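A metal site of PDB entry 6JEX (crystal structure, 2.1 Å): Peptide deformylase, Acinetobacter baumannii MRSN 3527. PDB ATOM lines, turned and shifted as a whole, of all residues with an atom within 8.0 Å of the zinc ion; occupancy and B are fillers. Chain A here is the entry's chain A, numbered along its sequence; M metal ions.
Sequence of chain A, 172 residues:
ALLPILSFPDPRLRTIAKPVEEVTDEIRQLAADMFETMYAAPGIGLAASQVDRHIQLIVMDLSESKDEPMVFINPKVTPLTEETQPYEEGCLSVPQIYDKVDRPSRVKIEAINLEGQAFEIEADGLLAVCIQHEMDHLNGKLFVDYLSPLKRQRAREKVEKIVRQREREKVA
ND1 of His 133 sits at hydrogen-bond distance from OE1 of Glu 89.
A ring nitrogen (NE2) of His 137 lies close to the side-chain amide oxygen (OE1) of Gln 50 (3.5 Å).
NE2 of Gln 50 sits close to SG of Cys 91 (3.7 Å).
The backbone NH (N) of Ser 93 lies close to the side-chain sulfur (SG) of Cys 91 (3.4 Å).
OE1 of Glu 134 lies close to OE1 of Gln 50 (3.3 Å).
The side-chain hydroxyl (OG) of Ser 93 is in hydrogen-bond range of the side-chain amide nitrogen (NE2) of Gln 50 (2.9 Å).
The side-chain amide oxygen of Gln 50 is in hydrogen-bond range of the backbone NH of Ala 47, at 2.9 Å.
NE2 of His 133 binds the zinc ion (2.0 Å).
The zinc ion is bound by NE2 of His 137.
SG of Cys 91 binds the zinc ion (2.2 Å).
The zinc ion has three donor atoms within binding distance.
Residues that only touch the zinc ion: Gln 50.
Of the 21 residues printed, 4 come within 4 Å of the zinc ion.
Along chain A the residues within 4 Å of the zinc ion span positions 50 to 137.
The nearest printed residue that does not touch the zinc ion is Glu 134 (4.03 Å).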
ATOM      1  N   ILE A   5       9.049  40.509 -14.571  1.00  0.00           N
ATOM      2  CA  ILE A   5       8.612  39.139 -14.276  1.00  0.00           C
ATOM      3  C   ILE A   5       8.507  38.947 -12.759  1.00  0.00           C
ATOM      4  O   ILE A   5       9.450  39.221 -12.052  1.00  0.00           O
ATOM      5  CB  ILE A   5       9.602  38.125 -14.882  1.00  0.00           C
ATOM      6  CG1 ILE A   5       9.681  38.333 -16.398  1.00  0.00           C
ATOM      7  CG2 ILE A   5       9.199  36.654 -14.580  1.00  0.00           C
ATOM      8  CD1 ILE A   5      10.761  37.500 -17.063  1.00  0.00           C
ATOM      9  N   LEU A  13       1.559  35.205  -8.033  1.00  0.00           N
ATOM     10  CA  LEU A  13       1.788  34.051  -8.927  1.00  0.00           C
ATOM     11  C   LEU A  13       0.767  32.955  -8.689  1.00  0.00           C
ATOM     12  O   LEU A  13       0.706  31.982  -9.451  1.00  0.00           O
ATOM     13  CB  LEU A  13       3.191  33.499  -8.772  1.00  0.00           C
ATOM     14  CG  LEU A  13       4.278  34.406  -9.389  1.00  0.00           C
ATOM     15  CD1 LEU A  13       5.666  34.110  -8.828  1.00  0.00           C
ATOM     16  CD2 LEU A  13       4.301  34.333 -10.890  1.00  0.00           C
ATOM     17  N   GLY A  45       9.360  29.939 -22.516  1.00  0.00           N
ATOM     18  CA  GLY A  45       7.943  29.933 -22.158  1.00  0.00           C
ATOM     19  C   GLY A  45       7.678  31.081 -21.177  1.00  0.00           C
ATOM     20  O   GLY A  45       8.474  31.342 -20.283  1.00  0.00           O
ATOM     21  N   LEU A  46       6.585  31.791 -21.352  1.00  0.00           N
ATOM     22  CA  LEU A  46       6.130  32.734 -20.367  1.00  0.00           C
ATOM     23  C   LEU A  46       4.633  32.838 -20.408  1.00  0.00           C
ATOM     24  O   LEU A  46       4.050  33.022 -21.486  1.00  0.00           O
ATOM     25  CB  LEU A  46       6.726  34.097 -20.658  1.00  0.00           C
ATOM     26  CG  LEU A  46       6.587  35.176 -19.582  1.00  0.00           C
ATOM     27  CD1 LEU A  46       7.433  34.857 -18.377  1.00  0.00           C
ATOM     28  CD2 LEU A  46       7.006  36.507 -20.232  1.00  0.00           C
ATOM     29  N   ALA A  47       4.000  32.746 -19.235  1.00  0.00           N
ATOM     30  CA  ALA A  47       2.546  32.874 -19.090  1.00  0.00           C
ATOM     31  C   ALA A  47       2.260  34.315 -18.631  1.00  0.00           C
ATOM     32  O   ALA A  47       3.086  34.964 -17.924  1.00  0.00           O
ATOM     33  CB  ALA A  47       2.007  31.922 -18.084  1.00  0.00           C
ATOM     34  N   GLN A  50       2.871  35.570 -15.095  1.00  0.00           N
ATOM     35  CA  GLN A  50       4.214  35.895 -14.695  1.00  0.00           C
ATOM     36  C   GLN A  50       4.607  37.380 -14.855  1.00  0.00           C
ATOM     37  O   GLN A  50       5.545  37.805 -14.218  1.00  0.00           O
ATOM     38  CB  GLN A  50       5.228  35.022 -15.457  1.00  0.00           C
ATOM     39  CG  GLN A  50       5.128  33.581 -15.074  1.00  0.00           C
ATOM     40  CD  GLN A  50       6.056  32.728 -15.855  1.00  0.00           C
ATOM     41  OE1 GLN A  50       5.658  32.194 -16.882  1.00  0.00           O
ATOM     42  NE2 GLN A  50       7.338  32.724 -15.466  1.00  0.00           N
ATOM     43  N   GLU A  89      13.095  20.998 -15.278  1.00  0.00           N
ATOM     44  CA  GLU A  89      12.370  22.278 -15.628  1.00  0.00           C
ATOM     45  C   GLU A  89      12.962  23.459 -14.903  1.00  0.00           C
ATOM     46  O   GLU A  89      13.437  23.310 -13.806  1.00  0.00           O
ATOM     47  CB  GLU A  89      10.925  22.196 -15.241  1.00  0.00           C
ATOM     48  CG  GLU A  89      10.126  21.304 -16.151  1.00  0.00           C
ATOM     49  CD  GLU A  89       8.666  21.177 -15.736  1.00  0.00           C
ATOM     50  OE1 GLU A  89       8.062  22.128 -15.142  1.00  0.00           O
ATOM     51  OE2 GLU A  89       8.114  20.113 -16.041  1.00  0.00           O
ATOM     52  N   GLY A  90      12.968  24.611 -15.573  1.00  0.00           N
ATOM     53  CA  GLY A  90      13.190  25.894 -14.973  1.00  0.00           C
ATOM     54  C   GLY A  90      11.993  26.801 -15.255  1.00  0.00           C
ATOM     55  O   GLY A  90      10.983  26.391 -15.865  1.00  0.00           O
ATOM     56  N   CYS A  91      12.122  28.035 -14.772  1.00  0.00           N
ATOM     57  CA  CYS A  91      11.041  28.993 -14.730  1.00  0.00           C
ATOM     58  C   CYS A  91      11.638  30.369 -14.531  1.00  0.00           C
ATOM     59  O   CYS A  91      12.406  30.560 -13.616  1.00  0.00           O
ATOM     60  CB  CYS A  91      10.056  28.716 -13.609  1.00  0.00           C
ATOM     61  SG  CYS A  91       8.542  29.715 -13.780  1.00  0.00           S
ATOM     62  N   LEU A  92      11.239  31.328 -15.350  1.00  0.00           N
ATOM     63  CA  LEU A  92      11.692  32.693 -15.208  1.00  0.00           C
ATOM     64  C   LEU A  92      11.167  33.314 -13.903  1.00  0.00           C
ATOM     65  O   LEU A  92      11.726  34.324 -13.447  1.00  0.00           O
ATOM     66  CB  LEU A  92      11.308  33.551 -16.421  1.00  0.00           C
ATOM     67  CG  LEU A  92      11.991  33.073 -17.704  1.00  0.00           C
ATOM     68  CD1 LEU A  92      11.447  33.901 -18.861  1.00  0.00           C
ATOM     69  CD2 LEU A  92      13.537  33.191 -17.609  1.00  0.00           C
ATOM     70  N   SER A  93      10.129  32.722 -13.312  1.00  0.00           N
ATOM     71  CA  SER A  93       9.578  33.242 -12.064  1.00  0.00           C
ATOM     72  C   SER A  93      10.167  32.496 -10.867  1.00  0.00           C
ATOM     73  O   SER A  93       9.742  32.725  -9.732  1.00  0.00           O
ATOM     74  CB  SER A  93       8.054  33.145 -12.025  1.00  0.00           C
ATOM     75  OG  SER A  93       7.479  34.105 -12.915  1.00  0.00           O
ATOM     76  N   VAL A  94      11.065  31.557 -11.135  1.00  0.00           N
ATOM     77  CA  VAL A  94      11.850  30.884 -10.077  1.00  0.00           C
ATOM     78  C   VAL A  94      13.294  30.968 -10.580  1.00  0.00           C
ATOM     79  O   VAL A  94      13.918  29.963 -10.920  1.00  0.00           O
ATOM     80  CB  VAL A  94      11.366  29.465  -9.861  1.00  0.00           C
ATOM     81  CG1 VAL A  94      11.998  28.900  -8.581  1.00  0.00           C
ATOM     82  CG2 VAL A  94       9.843  29.417  -9.781  1.00  0.00           C
ATOM     83  N   ARG A 103       5.703  14.558 -15.893  1.00  0.00           N
ATOM     84  CA  ARG A 103       4.376  14.935 -16.389  1.00  0.00           C
ATOM     85  C   ARG A 103       4.024  13.968 -17.515  1.00  0.00           C
ATOM     86  O   ARG A 103       4.929  13.509 -18.204  1.00  0.00           O
ATOM     87  CB  ARG A 103       4.427  16.335 -16.960  1.00  0.00           C
ATOM     88  CG  ARG A 103       4.890  17.427 -15.980  1.00  0.00           C
ATOM     89  CD  ARG A 103       4.908  18.798 -16.677  1.00  0.00           C
ATOM     90  NE  ARG A 103       5.396  19.918 -15.817  1.00  0.00           N
ATOM     91  CZ  ARG A 103       4.662  20.701 -15.021  1.00  0.00           C
ATOM     92  NH1 ARG A 103       3.368  20.487 -14.877  1.00  0.00           N
ATOM     93  NH2 ARG A 103       5.256  21.676 -14.310  1.00  0.00           N
ATOM     94  N   CYS A 130       6.345  21.847 -21.773  1.00  0.00           N
ATOM     95  CA  CYS A 130       6.290  23.313 -21.690  1.00  0.00           C
ATOM     96  C   CYS A 130       4.876  23.812 -21.590  1.00  0.00           C
ATOM     97  O   CYS A 130       4.597  24.682 -20.774  1.00  0.00           O
ATOM     98  CB  CYS A 130       7.031  23.984 -22.830  1.00  0.00           C
ATOM     99  SG  CYS A 130       7.234  25.774 -22.551  1.00  0.00           S
ATOM    100  N   HIS A 133       3.541  23.039 -18.054  1.00  0.00           N
ATOM    101  CA  HIS A 133       4.180  24.007 -17.117  1.00  0.00           C
ATOM    102  C   HIS A 133       3.478  25.344 -17.213  1.00  0.00           C
ATOM    103  O   HIS A 133       3.123  25.956 -16.192  1.00  0.00           O
ATOM    104  CB  HIS A 133       5.677  24.136 -17.453  1.00  0.00           C
ATOM    105  CG  HIS A 133       6.422  25.169 -16.672  1.00  0.00           C
ATOM    106  ND1 HIS A 133       7.403  24.849 -15.744  1.00  0.00           N
ATOM    107  CD2 HIS A 133       6.327  26.521 -16.669  1.00  0.00           C
ATOM    108  CE1 HIS A 133       7.872  25.956 -15.219  1.00  0.00           C
ATOM    109  NE2 HIS A 133       7.271  26.998 -15.795  1.00  0.00           N
ATOM    110  N   GLU A 134       3.242  25.796 -18.441  1.00  0.00           N
ATOM    111  CA  GLU A 134       2.659  27.125 -18.600  1.00  0.00           C
ATOM    112  C   GLU A 134       1.166  27.148 -18.215  1.00  0.00           C
ATOM    113  O   GLU A 134       0.727  28.102 -17.610  1.00  0.00           O
ATOM    114  CB  GLU A 134       2.906  27.700 -19.999  1.00  0.00           C
ATOM    115  CG  GLU A 134       4.386  27.855 -20.340  1.00  0.00           C
ATOM    116  CD  GLU A 134       5.120  28.779 -19.402  1.00  0.00           C
ATOM    117  OE1 GLU A 134       4.522  29.708 -18.813  1.00  0.00           O
ATOM    118  OE2 GLU A 134       6.354  28.585 -19.285  1.00  0.00           O
ATOM    119  N   ASP A 136      -0.099  25.375 -15.883  1.00  0.00           N
ATOM    120  CA  ASP A 136      -0.031  25.420 -14.434  1.00  0.00           C
ATOM    121  C   ASP A 136       0.049  26.866 -13.917  1.00  0.00           C
ATOM    122  O   ASP A 136      -0.625  27.189 -12.984  1.00  0.00           O
ATOM    123  CB  ASP A 136       1.156  24.608 -13.944  1.00  0.00           C
ATOM    124  CG  ASP A 136       0.830  23.109 -13.733  1.00  0.00           C
ATOM    125  OD1 ASP A 136      -0.295  22.691 -14.047  1.00  0.00           O
ATOM    126  OD2 ASP A 136       1.705  22.351 -13.215  1.00  0.00           O
ATOM    127  N   HIS A 137       0.825  27.740 -14.565  1.00  0.00           N
ATOM    128  CA  HIS A 137       0.837  29.202 -14.215  1.00  0.00           C
ATOM    129  C   HIS A 137      -0.540  29.866 -14.148  1.00  0.00           C
ATOM    130  O   HIS A 137      -0.848  30.603 -13.220  1.00  0.00           O
ATOM    131  CB  HIS A 137       1.739  30.030 -15.138  1.00  0.00           C
ATOM    132  CG  HIS A 137       3.185  29.936 -14.775  1.00  0.00           C
ATOM    133  ND1 HIS A 137       3.659  30.295 -13.519  1.00  0.00           N
ATOM    134  CD2 HIS A 137       4.261  29.521 -15.484  1.00  0.00           C
ATOM    135  CE1 HIS A 137       4.960  30.101 -13.481  1.00  0.00           C
ATOM    136  NE2 HIS A 137       5.340  29.573 -14.641  1.00  0.00           N
ATOM    137  N   LYS A 141      -0.271  27.739 -10.152  1.00  0.00           N
ATOM    138  CA  LYS A 141       0.705  26.720  -9.762  1.00  0.00           C
ATOM    139  C   LYS A 141       2.122  26.902 -10.364  1.00  0.00           C
ATOM    140  O   LYS A 141       2.270  27.272 -11.567  1.00  0.00           O
ATOM    141  CB  LYS A 141       0.198  25.354 -10.176  1.00  0.00           C
ATOM    142  CG  LYS A 141      -1.031  24.904  -9.424  1.00  0.00           C
ATOM    143  CD  LYS A 141      -1.493  23.534  -9.907  1.00  0.00           C
ATOM    144  CE  LYS A 141      -0.535  22.421  -9.464  1.00  0.00           C
ATOM    145  NZ  LYS A 141      -1.008  21.117  -9.983  1.00  0.00           N
ATOM    146  N   LEU A 142       3.134  26.589  -9.560  1.00  0.00           N
ATOM    147  CA  LEU A 142       4.537  26.669  -9.947  1.00  0.00           C
ATOM    148  C   LEU A 142       5.159  25.277  -9.907  1.00  0.00           C
ATOM    149  O   LEU A 142       4.692  24.423  -9.147  1.00  0.00           O
ATOM    150  CB  LEU A 142       5.324  27.610  -9.036  1.00  0.00           C
ATOM    151  CG  LEU A 142       4.879  29.054  -8.856  1.00  0.00           C
ATOM    152  CD1 LEU A 142       5.663  29.715  -7.710  1.00  0.00           C
ATOM    153  CD2 LEU A 142       5.091  29.803 -10.137  1.00  0.00           C
ATOM    154  N   PHE A 143       6.174  25.018 -10.733  1.00  0.00           N
ATOM    155  CA  PHE A 143       6.845  23.676 -10.744  1.00  0.00           C
ATOM    156  C   PHE A 143       7.498  23.244  -9.418  1.00  0.00           C
ATOM    157  O   PHE A 143       7.648  22.017  -9.152  1.00  0.00           O
ATOM    158  CB  PHE A 143       7.845  23.549 -11.900  1.00  0.00           C
ATOM    159  CG  PHE A 143       9.242  24.052 -11.587  1.00  0.00           C
ATOM    160  CD1 PHE A 143       9.591  25.406 -11.776  1.00  0.00           C
ATOM    161  CD2 PHE A 143      10.235  23.162 -11.131  1.00  0.00           C
ATOM    162  CE1 PHE A 143      10.891  25.842 -11.529  1.00  0.00           C
ATOM    163  CE2 PHE A 143      11.520  23.610 -10.873  1.00  0.00           C
ATOM    164  CZ  PHE A 143      11.856  24.950 -11.086  1.00  0.00           C
HETATM  165 ZN    ZN M   1       7.200  28.975 -15.367  1.00  0.00          ZN
